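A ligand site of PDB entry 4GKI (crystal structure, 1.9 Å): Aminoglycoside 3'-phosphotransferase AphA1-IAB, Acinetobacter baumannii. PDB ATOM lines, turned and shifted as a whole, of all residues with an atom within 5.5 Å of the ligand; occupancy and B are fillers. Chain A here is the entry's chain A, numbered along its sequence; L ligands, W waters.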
ATOM      1  N   ARG A 156     -26.321  18.592 -19.231  1.00  0.00           N
ATOM      2  CA  ARG A 156     -26.360  18.506 -17.773  1.00  0.00           C
ATOM      3  C   ARG A 156     -27.762  18.787 -17.264  1.00  0.00           C
ATOM      4  O   ARG A 156     -28.249  18.124 -16.342  1.00  0.00           O
ATOM      5  CB  ARG A 156     -25.317  19.443 -17.140  1.00  0.00           C
ATOM      6  CG  ARG A 156     -23.901  18.821 -17.226  1.00  0.00           C
ATOM      7  CD  ARG A 156     -22.806  19.656 -16.601  1.00  0.00           C
ATOM      8  NE  ARG A 156     -23.146  20.246 -15.299  1.00  0.00           N
ATOM      9  CZ  ARG A 156     -22.928  19.686 -14.110  1.00  0.00           C
ATOM     10  NH1 ARG A 156     -23.259  20.336 -12.998  1.00  0.00           N
ATOM     11  NH2 ARG A 156     -22.392  18.477 -14.035  1.00  0.00           N
ATOM     12  N   ASP A 163     -26.697  21.821 -10.362  1.00  0.00           N
ATOM     13  CA  ASP A 163     -26.836  22.015  -8.920  1.00  0.00           C
ATOM     14  C   ASP A 163     -27.681  23.255  -8.645  1.00  0.00           C
ATOM     15  O   ASP A 163     -27.150  24.358  -8.467  1.00  0.00           O
ATOM     16  CB  ASP A 163     -25.461  22.141  -8.236  1.00  0.00           C
ATOM     17  CG  ASP A 163     -25.568  22.244  -6.717  1.00  0.00           C
ATOM     18  OD1 ASP A 163     -26.703  22.250  -6.194  1.00  0.00           O
ATOM     19  OD2 ASP A 163     -24.502  22.316  -6.049  1.00  0.00           O
ATOM     20  N   ASP A 166     -27.108  25.908  -5.876  1.00  0.00           N
ATOM     21  CA  ASP A 166     -25.856  26.667  -5.884  1.00  0.00           C
ATOM     22  C   ASP A 166     -25.919  27.873  -6.832  1.00  0.00           C
ATOM     23  O   ASP A 166     -24.901  28.473  -7.128  1.00  0.00           O
ATOM     24  CB  ASP A 166     -24.683  25.745  -6.236  1.00  0.00           C
ATOM     25  CG  ASP A 166     -23.337  26.266  -5.724  1.00  0.00           C
ATOM     26  OD1 ASP A 166     -23.283  26.982  -4.700  1.00  0.00           O
ATOM     27  OD2 ASP A 166     -22.321  25.958  -6.388  1.00  0.00           O
ATOM     28  N   PHE A 167     -27.119  28.240  -7.277  1.00  0.00           N
ATOM     29  CA  PHE A 167     -27.280  29.417  -8.136  1.00  0.00           C
ATOM     30  C   PHE A 167     -26.886  30.679  -7.377  1.00  0.00           C
ATOM     31  O   PHE A 167     -27.046  30.753  -6.154  1.00  0.00           O
ATOM     32  CB  PHE A 167     -28.723  29.558  -8.633  1.00  0.00           C
ATOM     33  CG  PHE A 167     -29.144  28.500  -9.634  1.00  0.00           C
ATOM     34  CD1 PHE A 167     -28.199  27.671 -10.253  1.00  0.00           C
ATOM     35  CD2 PHE A 167     -30.483  28.344  -9.969  1.00  0.00           C
ATOM     36  CE1 PHE A 167     -28.615  26.700 -11.191  1.00  0.00           C
ATOM     37  CE2 PHE A 167     -30.906  27.393 -10.895  1.00  0.00           C
ATOM     38  CZ  PHE A 167     -29.975  26.574 -11.504  1.00  0.00           C
ATOM     39  N   ASP A 168     -26.378  31.682  -8.096  1.00  0.00           N
ATOM     40  CA  ASP A 168     -26.146  33.006  -7.496  1.00  0.00           C
ATOM     41  C   ASP A 168     -27.442  33.589  -6.907  1.00  0.00           C
ATOM     42  O   ASP A 168     -28.554  33.209  -7.295  1.00  0.00           O
ATOM     43  CB  ASP A 168     -25.586  33.991  -8.529  1.00  0.00           C
ATOM     44  CG  ASP A 168     -24.259  33.551  -9.090  1.00  0.00           C
ATOM     45  OD1 ASP A 168     -23.461  32.926  -8.350  1.00  0.00           O
ATOM     46  OD2 ASP A 168     -23.991  33.832 -10.283  1.00  0.00           O
ATOM     47  N   ASP A 169     -27.265  34.533  -5.989  1.00  0.00           N
ATOM     48  CA  ASP A 169     -28.382  35.145  -5.266  1.00  0.00           C
ATOM     49  C   ASP A 169     -29.548  35.575  -6.153  1.00  0.00           C
ATOM     50  O   ASP A 169     -30.722  35.302  -5.840  1.00  0.00           O
ATOM     51  CB  ASP A 169     -27.906  36.364  -4.467  1.00  0.00           C
ATOM     52  CG  ASP A 169     -29.050  37.085  -3.790  1.00  0.00           C
ATOM     53  OD1 ASP A 169     -29.582  36.520  -2.807  1.00  0.00           O
ATOM     54  OD2 ASP A 169     -29.449  38.186  -4.251  1.00  0.00           O
ATOM     55  N   ASP A 199     -12.446  28.048 -15.290  1.00  0.00           N
ATOM     56  CA  ASP A 199     -12.935  28.118 -13.914  1.00  0.00           C
ATOM     57  C   ASP A 199     -11.958  28.972 -13.114  1.00  0.00           C
ATOM     58  O   ASP A 199     -11.251  28.483 -12.213  1.00  0.00           O
ATOM     59  CB  ASP A 199     -13.075  26.718 -13.298  1.00  0.00           C
ATOM     60  CG  ASP A 199     -13.924  26.718 -12.040  1.00  0.00           C
ATOM     61  OD1 ASP A 199     -14.341  27.819 -11.626  1.00  0.00           O
ATOM     62  OD2 ASP A 199     -14.183  25.634 -11.466  1.00  0.00           O
ATOM     63  N   SER A 201     -11.490  30.831 -10.631  1.00  0.00           N
ATOM     64  CA  SER A 201     -12.038  31.241  -9.334  1.00  0.00           C
ATOM     65  C   SER A 201     -10.934  31.405  -8.294  1.00  0.00           C
ATOM     66  O   SER A 201      -9.792  30.999  -8.508  1.00  0.00           O
ATOM     67  CB  SER A 201     -13.031  30.192  -8.840  1.00  0.00           C
ATOM     68  OG  SER A 201     -12.335  29.016  -8.457  1.00  0.00           O
ATOM     69  N   ASP A 203     -10.410  29.783  -5.756  1.00  0.00           N
ATOM     70  CA  ASP A 203      -9.898  28.507  -5.261  1.00  0.00           C
ATOM     71  C   ASP A 203      -8.801  27.929  -6.150  1.00  0.00           C
ATOM     72  O   ASP A 203      -8.061  27.030  -5.733  1.00  0.00           O
ATOM     73  CB  ASP A 203     -11.030  27.493  -5.150  1.00  0.00           C
ATOM     74  CG  ASP A 203     -12.113  27.941  -4.193  1.00  0.00           C
ATOM     75  OD1 ASP A 203     -11.743  28.494  -3.131  1.00  0.00           O
ATOM     76  OD2 ASP A 203     -13.310  27.758  -4.494  1.00  0.00           O
ATOM     77  N   ASN A 204      -8.717  28.433  -7.387  1.00  0.00           N
ATOM     78  CA  ASN A 204      -7.843  27.802  -8.390  1.00  0.00           C
ATOM     79  C   ASN A 204      -6.588  28.585  -8.724  1.00  0.00           C
ATOM     80  O   ASN A 204      -5.864  28.231  -9.652  1.00  0.00           O
ATOM     81  CB  ASN A 204      -8.638  27.471  -9.668  1.00  0.00           C
ATOM     82  CG  ASN A 204      -9.635  26.353  -9.458  1.00  0.00           C
ATOM     83  OD1 ASN A 204      -9.441  25.493  -8.599  1.00  0.00           O
ATOM     84  ND2 ASN A 204     -10.701  26.338 -10.264  1.00  0.00           N
ATOM     85  N   ASP A 217      -6.468  23.158 -11.732  1.00  0.00           N
ATOM     86  CA  ASP A 217      -7.821  22.796 -12.187  1.00  0.00           C
ATOM     87  C   ASP A 217      -8.104  23.302 -13.623  1.00  0.00           C
ATOM     88  O   ASP A 217      -9.050  24.079 -13.855  1.00  0.00           O
ATOM     89  CB  ASP A 217      -8.855  23.356 -11.207  1.00  0.00           C
ATOM     90  CG  ASP A 217     -10.278  22.826 -11.457  1.00  0.00           C
ATOM     91  OD1 ASP A 217     -10.413  21.709 -12.017  1.00  0.00           O
ATOM     92  OD2 ASP A 217     -11.252  23.530 -11.105  1.00  0.00           O
ATOM     93  N   ASN A 235     -17.432  37.212  -9.852  1.00  0.00           N
ATOM     94  CA  ASN A 235     -18.409  36.583  -8.954  1.00  0.00           C
ATOM     95  C   ASN A 235     -17.798  36.266  -7.588  1.00  0.00           C
ATOM     96  O   ASN A 235     -18.326  36.692  -6.544  1.00  0.00           O
ATOM     97  CB  ASN A 235     -18.966  35.306  -9.610  1.00  0.00           C
ATOM     98  CG  ASN A 235     -20.326  34.897  -9.068  1.00  0.00           C
ATOM     99  OD1 ASN A 235     -21.062  35.716  -8.499  1.00  0.00           O
ATOM    100  ND2 ASN A 235     -20.677  33.636  -9.252  1.00  0.00           N
ATOM    101  N   CYS A 236     -16.649  35.602  -7.578  1.00  0.00           N
ATOM    102  CA  CYS A 236     -15.965  35.272  -6.318  1.00  0.00           C
ATOM    103  C   CYS A 236     -15.629  36.513  -5.482  1.00  0.00           C
ATOM    104  O   CYS A 236     -15.734  36.479  -4.254  1.00  0.00           O
ATOM    105  CB  CYS A 236     -14.675  34.497  -6.582  1.00  0.00           C
ATOM    106  SG  CYS A 236     -14.904  32.889  -7.345  1.00  0.00           S
ATOM    107  N   LEU A 237     -15.214  37.588  -6.142  1.00  0.00           N
ATOM    108  CA  LEU A 237     -14.809  38.792  -5.414  1.00  0.00           C
ATOM    109  C   LEU A 237     -15.992  39.438  -4.699  1.00  0.00           C
ATOM    110  O   LEU A 237     -15.826  40.226  -3.766  1.00  0.00           O
ATOM    111  CB  LEU A 237     -14.111  39.766  -6.372  1.00  0.00           C
ATOM    112  CG  LEU A 237     -12.709  39.289  -6.789  1.00  0.00           C
ATOM    113  CD1 LEU A 237     -12.161  40.107  -7.959  1.00  0.00           C
ATOM    114  CD2 LEU A 237     -11.755  39.308  -5.579  1.00  0.00           C
ATOM    115  N   GLU A 239     -17.788  38.012  -2.684  1.00  0.00           N
ATOM    116  CA  GLU A 239     -17.752  37.613  -1.272  1.00  0.00           C
ATOM    117  C   GLU A 239     -16.958  38.624  -0.448  1.00  0.00           C
ATOM    118  O   GLU A 239     -16.920  38.525   0.771  1.00  0.00           O
ATOM    119  CB  GLU A 239     -17.146  36.238  -1.070  1.00  0.00           C
ATOM    120  CG  GLU A 239     -18.100  35.095  -1.304  1.00  0.00           C
ATOM    121  CD  GLU A 239     -18.194  34.778  -2.764  1.00  0.00           C
ATOM    122  OE1 GLU A 239     -17.386  33.952  -3.240  1.00  0.00           O
ATOM    123  OE2 GLU A 239     -19.065  35.361  -3.447  1.00  0.00           O
ATOM    124  N   ASP A 269     -22.316  29.494 -16.146  1.00  0.00           N
ATOM    125  CA  ASP A 269     -21.651  28.733 -15.098  1.00  0.00           C
ATOM    126  C   ASP A 269     -22.627  28.069 -14.101  1.00  0.00           C
ATOM    127  O   ASP A 269     -22.248  27.134 -13.386  1.00  0.00           O
ATOM    128  CB  ASP A 269     -20.657  29.624 -14.329  1.00  0.00           C
ATOM    129  CG  ASP A 269     -19.594  28.806 -13.618  1.00  0.00           C
ATOM    130  OD1 ASP A 269     -19.089  27.828 -14.207  1.00  0.00           O
ATOM    131  OD2 ASP A 269     -19.237  29.158 -12.479  1.00  0.00           O
ATOM    132  N   GLU A 270     -23.866  28.548 -14.039  1.00  0.00           N
ATOM    133  CA  GLU A 270     -24.889  27.900 -13.190  1.00  0.00           C
ATOM    134  C   GLU A 270     -25.054  26.419 -13.534  1.00  0.00           C
ATOM    135  O   GLU A 270     -25.423  25.619 -12.669  1.00  0.00           O
ATOM    136  CB  GLU A 270     -26.254  28.590 -13.321  1.00  0.00           C
ATOM    137  CG  GLU A 270     -26.309  30.105 -12.970  1.00  0.00           C
ATOM    138  CD  GLU A 270     -26.072  30.425 -11.505  1.00  0.00           C
ATOM    139  OE1 GLU A 270     -25.344  29.657 -10.827  1.00  0.00           O
ATOM    140  OE2 GLU A 270     -26.597  31.454 -11.017  1.00  0.00           O
ATOM    141  N   PHE A 271     -24.773  26.057 -14.784  1.00  0.00           N
ATOM    142  CA  PHE A 271     -25.002  24.693 -15.257  1.00  0.00           C
ATOM    143  C   PHE A 271     -23.834  23.754 -14.985  1.00  0.00           C
ATOM    144  O   PHE A 271     -23.905  22.563 -15.275  1.00  0.00           O
ATOM    145  CB  PHE A 271     -25.318  24.683 -16.758  1.00  0.00           C
ATOM    146  CG  PHE A 271     -26.573  25.403 -17.105  1.00  0.00           C
ATOM    147  CD1 PHE A 271     -26.566  26.786 -17.246  1.00  0.00           C
ATOM    148  CD2 PHE A 271     -27.776  24.712 -17.256  1.00  0.00           C
ATOM    149  CE1 PHE A 271     -27.721  27.480 -17.519  1.00  0.00           C
ATOM    150  CE2 PHE A 271     -28.937  25.395 -17.549  1.00  0.00           C
ATOM    151  CZ  PHE A 271     -28.910  26.779 -17.680  1.00  0.00           C
ATOM    152  N   PHE A 272     -22.751  24.286 -14.443  1.00  0.00           N
ATOM    153  CA  PHE A 272     -21.554  23.469 -14.331  1.00  0.00           C
ATOM    154  C   PHE A 272     -21.111  23.193 -12.909  1.00  0.00           C
ATOM    155  O   PHE A 272     -20.068  22.544 -12.704  1.00  0.00           O
ATOM    156  CB  PHE A 272     -20.424  24.053 -15.184  1.00  0.00           C
ATOM    157  CG  PHE A 272     -20.712  23.971 -16.654  1.00  0.00           C
ATOM    158  CD1 PHE A 272     -20.495  22.792 -17.348  1.00  0.00           C
ATOM    159  CD2 PHE A 272     -21.270  25.049 -17.328  1.00  0.00           C
ATOM    160  CE1 PHE A 272     -20.794  22.693 -18.715  1.00  0.00           C
ATOM    161  CE2 PHE A 272     -21.576  24.955 -18.690  1.00  0.00           C
ATOM    162  CZ  PHE A 272     -21.339  23.777 -19.375  1.00  0.00           C
ATOM    163  OXT PHE A 272     -21.811  23.571 -11.970  1.00  0.00           O
HETATM  164  C1  LIG L   1     -18.683  25.703  -7.969  1.00  0.00           C
HETATM  165  C2  LIG L   1     -17.171  25.547  -7.988  1.00  0.00           C
HETATM  166  C3  LIG L   1     -16.693  24.912  -9.287  1.00  0.00           C
HETATM  167  C4  LIG L   1     -17.346  23.533  -9.412  1.00  0.00           C
HETATM  168  C5  LIG L   1     -18.861  23.726  -9.434  1.00  0.00           C
HETATM  169  C6  LIG L   1     -19.484  22.308  -9.515  1.00  0.00           C
HETATM  170  C7  LIG L   1     -22.146  29.477  -9.206  1.00  0.00           C
HETATM  171  C8  LIG L   1     -21.570  29.190  -7.862  1.00  0.00           C
HETATM  172  C9  LIG L   1     -20.205  28.492  -8.071  1.00  0.00           C
HETATM  173  C10 LIG L   1     -20.349  27.168  -8.868  1.00  0.00           C
HETATM  174  C11 LIG L   1     -20.924  27.530 -10.244  1.00  0.00           C
HETATM  175  C12 LIG L   1     -22.259  28.179 -10.044  1.00  0.00           C
HETATM  176  C13 LIG L   1     -21.428  30.403  -5.689  1.00  0.00           C
HETATM  177  C14 LIG L   1     -22.053  31.721  -5.166  1.00  0.00           C
HETATM  178  C15 LIG L   1     -21.312  32.952  -5.623  1.00  0.00           C
HETATM  179  C16 LIG L   1     -19.889  32.819  -5.122  1.00  0.00           C
HETATM  180  C17 LIG L   1     -19.273  31.572  -5.709  1.00  0.00           C
HETATM  181  C18 LIG L   1     -17.882  31.443  -5.137  1.00  0.00           C
HETATM  182  N1  LIG L   1     -20.957  22.364  -9.564  1.00  0.00           N
HETATM  183  N2  LIG L   1     -21.135  26.265 -10.973  1.00  0.00           N
HETATM  184  N3  LIG L   1     -23.466  30.081  -8.918  1.00  0.00           N
HETATM  185  N4  LIG L   1     -21.915  34.122  -4.961  1.00  0.00           N
HETATM  186  O1  LIG L   1     -19.275  24.369  -8.212  1.00  0.00           O
HETATM  187  O2  LIG L   1     -16.584  26.846  -7.841  1.00  0.00           O
HETATM  188  O3  LIG L   1     -15.274  24.796  -9.219  1.00  0.00           O
HETATM  189  O4  LIG L   1     -16.916  22.882 -10.603  1.00  0.00           O
HETATM  190  O5  LIG L   1     -19.057  26.540  -9.050  1.00  0.00           O
HETATM  191  O6  LIG L   1     -19.612  28.218  -6.776  1.00  0.00           O
HETATM  192  O7  LIG L   1     -21.513  30.455  -7.116  1.00  0.00           O
HETATM  193  O8  LIG L   1     -20.039  30.413  -5.300  1.00  0.00           O
HETATM  194  O9  LIG L   1     -23.414  31.789  -5.612  1.00  0.00           O
HETATM  195  O10 LIG L   1     -19.156  33.925  -5.609  1.00  0.00           O
HETATM  196  O11 LIG L   1     -17.316  30.254  -5.671  1.00  0.00           O
HETATM  197  O   HOH W   1     -12.196  24.802  -7.674  1.00  0.00           O
HETATM  198  O   HOH W   2     -22.072  22.887  -6.948  1.00  0.00           O
HETATM  199  O   HOH W   3     -22.136  19.872 -10.053  1.00  0.00           O
HETATM  200  O   HOH W   4     -18.808  28.307  -2.850  1.00  0.00           O
HETATM  201  O   HOH W   5     -22.362  31.947 -11.599  1.00  0.00           O
HETATM  202  O   HOH W   6     -16.909  24.253 -13.370  1.00  0.00           O
HETATM  203  O   HOH W   7     -18.613  25.906 -12.220  1.00  0.00           O
HETATM  204  O   HOH W   8     -22.826  24.745  -9.221  1.00  0.00           O
HETATM  205  O   HOH W   9     -24.710  35.128  -5.172  1.00  0.00           O
HETATM  206  O   HOH W  10     -14.509  30.021  -5.435  1.00  0.00           O
HETATM  207  O   HOH W  11     -17.092  26.938  -4.981  1.00  0.00           O
HETATM  208  O   HOH W  12     -20.994  36.659  -5.920  1.00  0.00           O
HETATM  209  O   HOH W  13     -20.751  27.284  -4.260  1.00  0.00           O
HETATM  210  O   HOH W  14     -15.724  20.238 -10.191  1.00  0.00           O
HETATM  211  O   HOH W  15     -16.885  28.244 -10.743  1.00  0.00           O
HETATM  212  O   HOH W  16     -13.898  27.006  -7.317  1.00  0.00           O
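OE2 of Glu 239 lies within salt-bridge range of N4 of the ligand (3.5 Å). O3 of the ligand lies within hydrogen-bond range of OD2 of Asp 199, 2.6 Å away. OE1 of Glu 270 is in salt-bridge range of N3 of the ligand (2.7 Å). The backbone carbonyl oxygen (O) of Asp 269 lies within hydrogen-bond range of a nitrogen (N2) of the ligand, 2.8 Å away. A nitrogen (N2) of the ligand is in salt-bridge range of the side-chain carboxylate (OD2) of Asp 269, at 3.8 Å. A nitrogen (N3) of the ligand lies within hydrogen-bond range of the backbone carbonyl oxygen (O) of Asp 166 (2.8 Å). N1 of the ligand lies within salt-bridge range of OXT of Phe 272 (2.8 Å). A nitrogen (N3) of the ligand lies close to the backbone NH (N) of Asp 168. The side-chain carboxylate (OD1) of Asp 168 lies within salt-bridge range of a nitrogen (N3) of the ligand. The backbone carbonyl oxygen (O) of Asn 235 sits at hydrogen-bond distance from an oxygen (O10) of the ligand.
The backbone carbonyl oxygen (O) of Asp 199 is in hydrogen-bond range of the side-chain amide nitrogen (ND2) of Asn 204, at 2.9 Å. OE2 of Glu 270 is in hydrogen-bond range of N of Asp 168, 2.9 Å away. The chain-end carboxylate (OXT) of Phe 272 lies within salt-bridge range of the guanidinium group (NH1) of Arg 156 (3.7 Å). OD1 of Asp 168 sits at hydrogen-bond distance from ND2 of Asn 235 (3.0 Å).
Merely in contact with the ligand: Cys 236 and Phe 167. The nearest printed residue that does not touch the ligand is Arg 156 (4.6 Å).
Water W16 lies within hydrogen-bond range of O2 of the ligand (2.7 Å), OG of Ser 201 (2.8 Å) and OD2 of Asp 203 (3.0 Å). Water W3 bridges N1 of the ligand (2.8 Å) and NH1 of Arg 156 (3.2 Å). Water W12 lies within hydrogen-bond range of the backbone carbonyl oxygen of Asn 235 (2.7 Å), a nitrogen (N4) of the ligand (2.9 Å) and the side-chain carboxylate of Glu 239 (3.4 Å). Water W2 lies within hydrogen-bond range of OD2 of Asp 163 (2.7 Å), N1 of the ligand (2.9 Å) and OD2 of Asp 166 (3.1 Å). Water W13 lies within hydrogen-bond range of OD1 of Asp 166 (2.6 Å) and O6 of the ligand (2.9 Å). Water W1 lies within hydrogen-bond range of OD1 of Asn 204 (3.0 Å) and O3 of the ligand (3.4 Å).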
